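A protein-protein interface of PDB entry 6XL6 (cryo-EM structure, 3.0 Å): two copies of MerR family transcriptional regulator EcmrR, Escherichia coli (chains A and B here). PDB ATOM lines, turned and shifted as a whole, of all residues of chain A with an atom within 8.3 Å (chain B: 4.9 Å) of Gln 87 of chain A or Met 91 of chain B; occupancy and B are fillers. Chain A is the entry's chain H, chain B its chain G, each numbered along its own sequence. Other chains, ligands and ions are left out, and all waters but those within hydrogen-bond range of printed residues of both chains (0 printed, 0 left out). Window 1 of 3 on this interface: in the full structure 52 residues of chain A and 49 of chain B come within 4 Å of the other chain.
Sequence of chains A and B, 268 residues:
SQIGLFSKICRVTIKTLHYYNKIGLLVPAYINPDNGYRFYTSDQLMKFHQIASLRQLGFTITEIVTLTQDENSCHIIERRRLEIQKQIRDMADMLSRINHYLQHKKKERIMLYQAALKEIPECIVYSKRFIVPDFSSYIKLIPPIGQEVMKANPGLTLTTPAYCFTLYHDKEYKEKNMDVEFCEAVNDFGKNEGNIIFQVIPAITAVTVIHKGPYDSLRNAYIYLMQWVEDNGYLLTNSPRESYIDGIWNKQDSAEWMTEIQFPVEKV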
ATOM      1  N   LEU A  57     -15.665   5.250  -5.252  1.00  0.00           N
ATOM      2  CA  LEU A  57     -15.895   3.906  -4.740  1.00  0.00           C
ATOM      3  C   LEU A  57     -17.062   3.846  -3.767  1.00  0.00           C
ATOM      4  O   LEU A  57     -17.397   2.760  -3.289  1.00  0.00           O
ATOM      5  CB  LEU A  57     -14.631   3.382  -4.056  1.00  0.00           C
ATOM      6  CG  LEU A  57     -13.686   2.472  -4.841  1.00  0.00           C
ATOM      7  CD1 LEU A  57     -13.396   3.038  -6.208  1.00  0.00           C
ATOM      8  CD2 LEU A  57     -12.394   2.301  -4.070  1.00  0.00           C
ATOM      9  N   GLY A  58     -17.685   4.981  -3.466  1.00  0.00           N
ATOM     10  CA  GLY A  58     -18.835   5.010  -2.592  1.00  0.00           C
ATOM     11  C   GLY A  58     -18.548   5.360  -1.153  1.00  0.00           C
ATOM     12  O   GLY A  58     -19.489   5.430  -0.354  1.00  0.00           O
ATOM     13  N   ARG A  80     -16.906  -1.730   3.493  1.00  0.00           N
ATOM     14  CA  ARG A  80     -17.589  -1.122   2.357  1.00  0.00           C
ATOM     15  C   ARG A  80     -17.846  -2.137   1.252  1.00  0.00           C
ATOM     16  O   ARG A  80     -18.857  -2.044   0.553  1.00  0.00           O
ATOM     17  CB  ARG A  80     -16.768   0.058   1.833  1.00  0.00           C
ATOM     18  CG  ARG A  80     -17.259   0.678   0.535  1.00  0.00           C
ATOM     19  CD  ARG A  80     -18.601   1.356   0.693  1.00  0.00           C
ATOM     20  NE  ARG A  80     -19.257   1.531  -0.596  1.00  0.00           N
ATOM     21  CZ  ARG A  80     -20.513   1.935  -0.743  1.00  0.00           C
ATOM     22  NH1 ARG A  80     -21.032   2.068  -1.953  1.00  0.00           N
ATOM     23  NH2 ARG A  80     -21.248   2.208   0.321  1.00  0.00           N
ATOM     24  N   ARG A  81     -16.966  -3.126   1.098  1.00  0.00           N
ATOM     25  CA  ARG A  81     -17.183  -4.161   0.091  1.00  0.00           C
ATOM     26  C   ARG A  81     -18.393  -5.023   0.430  1.00  0.00           C
ATOM     27  O   ARG A  81     -19.224  -5.318  -0.439  1.00  0.00           O
ATOM     28  CB  ARG A  81     -15.932  -5.022  -0.045  1.00  0.00           C
ATOM     29  CG  ARG A  81     -16.086  -6.183  -0.997  1.00  0.00           C
ATOM     30  CD  ARG A  81     -14.806  -6.982  -1.086  1.00  0.00           C
ATOM     31  NE  ARG A  81     -15.018  -8.268  -1.735  1.00  0.00           N
ATOM     32  CZ  ARG A  81     -15.397  -9.366  -1.095  1.00  0.00           C
ATOM     33  NH1 ARG A  81     -15.603  -9.332   0.214  1.00  0.00           N
ATOM     34  NH2 ARG A  81     -15.568 -10.500  -1.761  1.00  0.00           N
ATOM     35  N   LEU A  82     -18.510  -5.438   1.692  1.00  0.00           N
ATOM     36  CA  LEU A  82     -19.689  -6.191   2.112  1.00  0.00           C
ATOM     37  C   LEU A  82     -20.947  -5.340   2.002  1.00  0.00           C
ATOM     38  O   LEU A  82     -22.019  -5.845   1.642  1.00  0.00           O
ATOM     39  CB  LEU A  82     -19.508  -6.700   3.540  1.00  0.00           C
ATOM     40  CG  LEU A  82     -18.291  -7.588   3.802  1.00  0.00           C
ATOM     41  CD1 LEU A  82     -18.205  -7.947   5.274  1.00  0.00           C
ATOM     42  CD2 LEU A  82     -18.336  -8.840   2.946  1.00  0.00           C
ATOM     43  N   GLU A  83     -20.829  -4.044   2.293  1.00  0.00           N
ATOM     44  CA  GLU A  83     -21.961  -3.138   2.127  1.00  0.00           C
ATOM     45  C   GLU A  83     -22.394  -3.053   0.670  1.00  0.00           C
ATOM     46  O   GLU A  83     -23.591  -3.050   0.372  1.00  0.00           O
ATOM     47  CB  GLU A  83     -21.598  -1.754   2.662  1.00  0.00           C
ATOM     48  CG  GLU A  83     -22.778  -0.824   2.824  1.00  0.00           C
ATOM     49  CD  GLU A  83     -22.368   0.632   2.809  1.00  0.00           C
ATOM     50  OE1 GLU A  83     -21.307   0.955   3.380  1.00  0.00           O
ATOM     51  OE2 GLU A  83     -23.105   1.455   2.224  1.00  0.00           O
ATOM     52  N   ILE A  84     -21.434  -2.984  -0.253  1.00  0.00           N
ATOM     53  CA  ILE A  84     -21.760  -2.935  -1.675  1.00  0.00           C
ATOM     54  C   ILE A  84     -22.414  -4.236  -2.118  1.00  0.00           C
ATOM     55  O   ILE A  84     -23.353  -4.234  -2.922  1.00  0.00           O
ATOM     56  CB  ILE A  84     -20.498  -2.626  -2.502  1.00  0.00           C
ATOM     57  CG1 ILE A  84     -20.063  -1.182  -2.294  1.00  0.00           C
ATOM     58  CG2 ILE A  84     -20.745  -2.858  -3.972  1.00  0.00           C
ATOM     59  CD1 ILE A  84     -18.750  -0.853  -2.954  1.00  0.00           C
ATOM     60  N   GLN A  85     -21.929  -5.369  -1.603  1.00  0.00           N
ATOM     61  CA  GLN A  85     -22.550  -6.647  -1.940  1.00  0.00           C
ATOM     62  C   GLN A  85     -23.992  -6.701  -1.454  1.00  0.00           C
ATOM     63  O   GLN A  85     -24.883  -7.176  -2.171  1.00  0.00           O
ATOM     64  CB  GLN A  85     -21.744  -7.799  -1.346  1.00  0.00           C
ATOM     65  CG  GLN A  85     -20.439  -8.069  -2.058  1.00  0.00           C
ATOM     66  CD  GLN A  85     -19.726  -9.284  -1.514  1.00  0.00           C
ATOM     67  OE1 GLN A  85     -19.775 -10.362  -2.105  1.00  0.00           O
ATOM     68  NE2 GLN A  85     -19.053  -9.119  -0.383  1.00  0.00           N
ATOM     69  N   LYS A  86     -24.244  -6.200  -0.243  1.00  0.00           N
ATOM     70  CA  LYS A  86     -25.611  -6.143   0.263  1.00  0.00           C
ATOM     71  C   LYS A  86     -26.474  -5.212  -0.579  1.00  0.00           C
ATOM     72  O   LYS A  86     -27.638  -5.518  -0.860  1.00  0.00           O
ATOM     73  CB  LYS A  86     -25.613  -5.697   1.723  1.00  0.00           C
ATOM     74  CG  LYS A  86     -26.990  -5.685   2.355  1.00  0.00           C
ATOM     75  CD  LYS A  86     -26.932  -5.239   3.802  1.00  0.00           C
ATOM     76  CE  LYS A  86     -28.291  -5.367   4.461  1.00  0.00           C
ATOM     77  NZ  LYS A  86     -28.292  -4.795   5.833  1.00  0.00           N
ATOM     78  N   GLN A  87     -25.919  -4.071  -0.994  1.00  0.00           N
ATOM     79  CA  GLN A  87     -26.674  -3.139  -1.824  1.00  0.00           C
ATOM     80  C   GLN A  87     -27.029  -3.759  -3.168  1.00  0.00           C
ATOM     81  O   GLN A  87     -28.135  -3.558  -3.673  1.00  0.00           O
ATOM     82  CB  GLN A  87     -25.883  -1.848  -2.028  1.00  0.00           C
ATOM     83  CG  GLN A  87     -25.699  -1.014  -0.774  1.00  0.00           C
ATOM     84  CD  GLN A  87     -26.975  -0.870   0.023  1.00  0.00           C
ATOM     85  OE1 GLN A  87     -27.969  -0.334  -0.466  1.00  0.00           O
ATOM     86  NE2 GLN A  87     -26.957  -1.350   1.260  1.00  0.00           N
ATOM     87  N   ILE A  88     -26.111  -4.526  -3.754  1.00  0.00           N
ATOM     88  CA  ILE A  88     -26.404  -5.195  -5.019  1.00  0.00           C
ATOM     89  C   ILE A  88     -27.475  -6.259  -4.826  1.00  0.00           C
ATOM     90  O   ILE A  88     -28.390  -6.398  -5.650  1.00  0.00           O
ATOM     91  CB  ILE A  88     -25.121  -5.796  -5.621  1.00  0.00           C
ATOM     92  CG1 ILE A  88     -24.119  -4.700  -5.956  1.00  0.00           C
ATOM     93  CG2 ILE A  88     -25.439  -6.592  -6.871  1.00  0.00           C
ATOM     94  CD1 ILE A  88     -22.857  -5.217  -6.581  1.00  0.00           C
ATOM     95  N   ARG A  89     -27.375  -7.033  -3.742  1.00  0.00           N
ATOM     96  CA  ARG A  89     -28.363  -8.075  -3.486  1.00  0.00           C
ATOM     97  C   ARG A  89     -29.744  -7.489  -3.221  1.00  0.00           C
ATOM     98  O   ARG A  89     -30.755  -8.118  -3.550  1.00  0.00           O
ATOM     99  CB  ARG A  89     -27.909  -8.938  -2.311  1.00  0.00           C
ATOM    100  CG  ARG A  89     -28.730 -10.195  -2.095  1.00  0.00           C
ATOM    101  CD  ARG A  89     -28.087 -11.092  -1.053  1.00  0.00           C
ATOM    102  NE  ARG A  89     -27.587 -10.331   0.087  1.00  0.00           N
ATOM    103  CZ  ARG A  89     -26.309 -10.279   0.446  1.00  0.00           C
ATOM    104  NH1 ARG A  89     -25.397 -10.950  -0.246  1.00  0.00           N
ATOM    105  NH2 ARG A  89     -25.940  -9.562   1.498  1.00  0.00           N
ATOM    106  N   ASP A  90     -29.808  -6.291  -2.638  1.00  0.00           N
ATOM    107  CA  ASP A  90     -31.095  -5.634  -2.430  1.00  0.00           C
ATOM    108  C   ASP A  90     -31.613  -5.010  -3.719  1.00  0.00           C
ATOM    109  O   ASP A  90     -32.821  -5.013  -3.981  1.00  0.00           O
ATOM    110  CB  ASP A  90     -30.977  -4.579  -1.334  1.00  0.00           C
ATOM    111  CG  ASP A  90     -30.497  -5.155  -0.020  1.00  0.00           C
ATOM    112  OD1 ASP A  90     -30.280  -6.382   0.045  1.00  0.00           O
ATOM    113  OD2 ASP A  90     -30.332  -4.381   0.946  1.00  0.00           O
ATOM    114  N   MET A  91     -30.715  -4.459  -4.537  1.00  0.00           N
ATOM    115  CA  MET A  91     -31.140  -3.802  -5.766  1.00  0.00           C
ATOM    116  C   MET A  91     -31.664  -4.808  -6.779  1.00  0.00           C
ATOM    117  O   MET A  91     -32.632  -4.529  -7.492  1.00  0.00           O
ATOM    118  CB  MET A  91     -29.989  -2.994  -6.359  1.00  0.00           C
ATOM    119  CG  MET A  91     -29.764  -1.649  -5.701  1.00  0.00           C
ATOM    120  SD  MET A  91     -31.218  -0.593  -5.771  1.00  0.00           S
ATOM    121  CE  MET A  91     -31.155   0.161  -4.148  1.00  0.00           C
ATOM    122  N   ALA A  92     -31.033  -5.980  -6.870  1.00  0.00           N
ATOM    123  CA  ALA A  92     -31.557  -7.012  -7.760  1.00  0.00           C
ATOM    124  C   ALA A  92     -32.931  -7.486  -7.309  1.00  0.00           C
ATOM    125  O   ALA A  92     -33.815  -7.727  -8.146  1.00  0.00           O
ATOM    126  CB  ALA A  92     -30.586  -8.188  -7.833  1.00  0.00           C
ATOM    127  N   ASP A  93     -33.130  -7.601  -5.995  1.00  0.00           N
ATOM    128  CA  ASP A  93     -34.448  -7.911  -5.452  1.00  0.00           C
ATOM    129  C   ASP A  93     -35.466  -6.856  -5.854  1.00  0.00           C
ATOM    130  O   ASP A  93     -36.547  -7.182  -6.352  1.00  0.00           O
ATOM    131  CB  ASP A  93     -34.369  -8.028  -3.933  1.00  0.00           C
ATOM    132  CG  ASP A  93     -35.708  -8.317  -3.304  1.00  0.00           C
ATOM    133  OD1 ASP A  93     -36.205  -9.453  -3.443  1.00  0.00           O
ATOM    134  OD2 ASP A  93     -36.266  -7.402  -2.664  1.00  0.00           O
ATOM    135  N   MET A  94     -35.134  -5.580  -5.635  1.00  0.00           N
ATOM    136  CA  MET A  94     -36.028  -4.491  -6.015  1.00  0.00           C
ATOM    137  C   MET A  94     -36.334  -4.507  -7.504  1.00  0.00           C
ATOM    138  O   MET A  94     -37.459  -4.204  -7.908  1.00  0.00           O
ATOM    139  CB  MET A  94     -35.418  -3.146  -5.626  1.00  0.00           C
ATOM    140  CG  MET A  94     -35.401  -2.870  -4.139  1.00  0.00           C
ATOM    141  SD  MET A  94     -34.651  -1.280  -3.756  1.00  0.00           S
ATOM    142  CE  MET A  94     -34.808  -1.254  -1.974  1.00  0.00           C
ATOM    143  N   GLN B  87     -28.491   2.084 -11.167  1.00  0.00           N
ATOM    144  CA  GLN B  87     -27.835   1.893  -9.881  1.00  0.00           C
ATOM    145  C   GLN B  87     -27.208   0.516  -9.755  1.00  0.00           C
ATOM    146  O   GLN B  87     -26.182   0.381  -9.090  1.00  0.00           O
ATOM    147  CB  GLN B  87     -28.822   2.110  -8.737  1.00  0.00           C
ATOM    148  CG  GLN B  87     -29.232   3.552  -8.528  1.00  0.00           C
ATOM    149  CD  GLN B  87     -30.164   3.721  -7.347  1.00  0.00           C
ATOM    150  OE1 GLN B  87     -30.522   2.752  -6.682  1.00  0.00           O
ATOM    151  NE2 GLN B  87     -30.564   4.958  -7.082  1.00  0.00           N
ATOM    152  N   ILE B  88     -27.791  -0.503 -10.386  1.00  0.00           N
ATOM    153  CA  ILE B  88     -27.193  -1.833 -10.357  1.00  0.00           C
ATOM    154  C   ILE B  88     -25.887  -1.842 -11.136  1.00  0.00           C
ATOM    155  O   ILE B  88     -24.888  -2.424 -10.692  1.00  0.00           O
ATOM    156  CB  ILE B  88     -28.186  -2.878 -10.897  1.00  0.00           C
ATOM    157  CG1 ILE B  88     -29.265  -3.170  -9.859  1.00  0.00           C
ATOM    158  CG2 ILE B  88     -27.472  -4.163 -11.273  1.00  0.00           C
ATOM    159  CD1 ILE B  88     -30.195  -4.284 -10.248  1.00  0.00           C
ATOM    160  N   ARG B  89     -25.870  -1.201 -12.307  1.00  0.00           N
ATOM    161  CA  ARG B  89     -24.624  -1.075 -13.057  1.00  0.00           C
ATOM    162  C   ARG B  89     -23.566  -0.336 -12.249  1.00  0.00           C
ATOM    163  O   ARG B  89     -22.408  -0.767 -12.180  1.00  0.00           O
ATOM    164  CB  ARG B  89     -24.871  -0.357 -14.381  1.00  0.00           C
ATOM    165  CG  ARG B  89     -25.531  -1.207 -15.440  1.00  0.00           C
ATOM    166  CD  ARG B  89     -25.686  -0.429 -16.733  1.00  0.00           C
ATOM    167  NE  ARG B  89     -26.583  -1.103 -17.665  1.00  0.00           N
ATOM    168  CZ  ARG B  89     -27.867  -0.795 -17.815  1.00  0.00           C
ATOM    169  NH1 ARG B  89     -28.613  -1.461 -18.683  1.00  0.00           N
ATOM    170  NH2 ARG B  89     -28.405   0.179 -17.093  1.00  0.00           N
ATOM    171  N   ASP B  90     -23.951   0.774 -11.615  1.00  0.00           N
ATOM    172  CA  ASP B  90     -22.987   1.550 -10.841  1.00  0.00           C
ATOM    173  C   ASP B  90     -22.496   0.778  -9.623  1.00  0.00           C
ATOM    174  O   ASP B  90     -21.323   0.877  -9.251  1.00  0.00           O
ATOM    175  CB  ASP B  90     -23.604   2.882 -10.420  1.00  0.00           C
ATOM    176  CG  ASP B  90     -24.060   3.713 -11.603  1.00  0.00           C
ATOM    177  OD1 ASP B  90     -23.778   3.323 -12.754  1.00  0.00           O
ATOM    178  OD2 ASP B  90     -24.706   4.757 -11.379  1.00  0.00           O
ATOM    179  N   MET B  91     -23.368  -0.017  -9.004  1.00  0.00           N
ATOM    180  CA  MET B  91     -22.968  -0.782  -7.830  1.00  0.00           C
ATOM    181  C   MET B  91     -22.057  -1.940  -8.209  1.00  0.00           C
ATOM    182  O   MET B  91     -21.111  -2.251  -7.481  1.00  0.00           O
ATOM    183  CB  MET B  91     -24.206  -1.287  -7.091  1.00  0.00           C
ATOM    184  CG  MET B  91     -24.661  -0.384  -5.963  1.00  0.00           C
ATOM    185  SD  MET B  91     -23.440  -0.293  -4.645  1.00  0.00           S
ATOM    186  CE  MET B  91     -24.150   0.977  -3.605  1.00  0.00           C
ATOM    187  N   ALA B  92     -22.320  -2.590  -9.343  1.00  0.00           N
ATOM    188  CA  ALA B  92     -21.404  -3.617  -9.823  1.00  0.00           C
ATOM    189  C   ALA B  92     -20.049  -3.024 -10.179  1.00  0.00           C
ATOM    190  O   ALA B  92     -19.009  -3.639  -9.903  1.00  0.00           O
ATOM    191  CB  ALA B  92     -22.005  -4.336 -11.028  1.00  0.00           C
ATOM    192  N   ASP B  93     -20.042  -1.831 -10.776  1.00  0.00           N
ATOM    193  CA  ASP B  93     -18.786  -1.140 -11.039  1.00  0.00           C
ATOM    194  C   ASP B  93     -18.038  -0.860  -9.744  1.00  0.00           C
ATOM    195  O   ASP B  93     -16.839  -1.132  -9.643  1.00  0.00           O
ATOM    196  CB  ASP B  93     -19.054   0.158 -11.800  1.00  0.00           C
ATOM    197  CG  ASP B  93     -17.856   0.623 -12.596  1.00  0.00           C
ATOM    198  OD1 ASP B  93     -17.286   1.678 -12.253  1.00  0.00           O
ATOM    199  OD2 ASP B  93     -17.484  -0.066 -13.569  1.00  0.00           O
ATOM    200  N   MET B  94     -18.737  -0.322  -8.740  1.00  0.00           N
ATOM    201  CA  MET B  94     -18.120  -0.057  -7.443  1.00  0.00           C
ATOM    202  C   MET B  94     -17.565  -1.328  -6.816  1.00  0.00           C
ATOM    203  O   MET B  94     -16.483  -1.314  -6.220  1.00  0.00           O
ATOM    204  CB  MET B  94     -19.135   0.587  -6.500  1.00  0.00           C
ATOM    205  CG  MET B  94     -19.353   2.070  -6.719  1.00  0.00           C
ATOM    206  SD  MET B  94     -20.325   2.807  -5.397  1.00  0.00           S
ATOM    207  CE  MET B  94     -20.403   4.506  -5.946  1.00  0.00           C
ATOM    208  N   LEU B  95     -18.296  -2.436  -6.940  1.00  0.00           N
ATOM    209  CA  LEU B  95     -17.842  -3.697  -6.365  1.00  0.00           C
ATOM    210  C   LEU B  95     -16.567  -4.176  -7.040  1.00  0.00           C
ATOM    211  O   LEU B  95     -15.624  -4.609  -6.371  1.00  0.00           O
ATOM    212  CB  LEU B  95     -18.937  -4.755  -6.482  1.00  0.00           C
ATOM    213  CG  LEU B  95     -18.638  -6.076  -5.776  1.00  0.00           C
ATOM    214  CD1 LEU B  95     -18.501  -5.854  -4.286  1.00  0.00           C
ATOM    215  CD2 LEU B  95     -19.717  -7.099  -6.071  1.00  0.00           C
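Gly 58 of chain A touches Met 94 of chain B (N to CE, 3.7 Å). Met 91 of chain B touches Arg 80 of chain A. CD1 of Ile 84 of chain A touches CB of Met 94 of chain B (3.8 Å). CG2 of Ile 84 of chain A touches CB of Leu 95 of chain B, 3.6 Å away. CG of Gln 85 of chain A touches CD1 of Leu 95 of chain B, 3.7 Å away. Ile 88 of chain A touches Met 91 of chain B (CD1 to O, 3.6 Å). Ile 88 of chain A touches Ala 92 of chain B (CD1 to N, 3.8 Å). CD2 of Leu 95 of chain B touches CD1 of Ile 88 of chain A, at 3.7 Å. Ile 88 of chain B touches Met 91 of chain A (CG1 to CB, 3.6 Å). Ala 92 of chain A touches Ile 88 of chain B.
Gln 87 of chain A touches Met 91 of chain B, and with the chains exchanged Met 91 of chain A touches Gln 87 of chain B. Ile 88 of chain A touches Met 91 of chain B, and with the chains exchanged Met 91 of chain A touches Ile 88 of chain B. Ile 88 of chain A touches Ala 92 of chain B, and with the chains exchanged Ala 92 of chain A touches Ile 88 of chain B. Positions printed for both chains: 87, 88, 89, 90, 91, 92, 93 and 94.
Hydrophobic or aromatic side chains of chain A that line the printed part of chain B: Ile 84, Ile 88 and Met 91. Along chain A the printed residues that touch a printed residue of chain B span positions 57 to 92. Hydrophobic or aromatic side chains of chain B that line the printed part of chain A: Ile 88, Met 91, Met 94 and Leu 95.
Of the printed residues of chain B, Leu 57 of chain A touches Met 94 (3.6 Å). Of the printed residues of chain B, Arg 81 of chain A touches Leu 95 (3.95 Å). Of chain B, only Met 91 comes within 4 Å of Gln 87 of chain A. Of the printed residues of chain B, Ile 88 of chain A touches Met 91, Ala 92 and Leu 95. Asp 90 of chain A touches none of the printed residues of chain B. Printed residues of chain A within 4 Å of Gln 87 of chain B: Met 91 (3.5 Å). Of the printed residues of chain A, Met 91 of chain B touches Arg 80, Ile 84, Gln 87 and Ile 88. The nearest printed residue of chain B that does not touch Gln 87 of chain A is Ile 88 of chain B (6.3 Å).
The backbone carbonyl oxygen (O) of Leu 57 of chain A sits at hydrogen-bond distance from the guanidinium group (NE) of Arg 80 of chain A. The guanidinium group (NH2) of Arg 80 of chain A is in salt-bridge range of the side-chain carboxylate (OE2) of Glu 83 of chain A (2.8 Å).
The side-chain sulfur of Met 91 of chain A sits close to the side-chain amide oxygen of Gln 87 of chain B, 3.5 Å away. NH1 of Arg 80 of chain A sits at hydrogen-bond distance from SD of Met 94 of chain B (3.6 Å). The side-chain sulfur of Met 94 of chain B sits close to the backbone carbonyl oxygen of Leu 57 of chain A.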
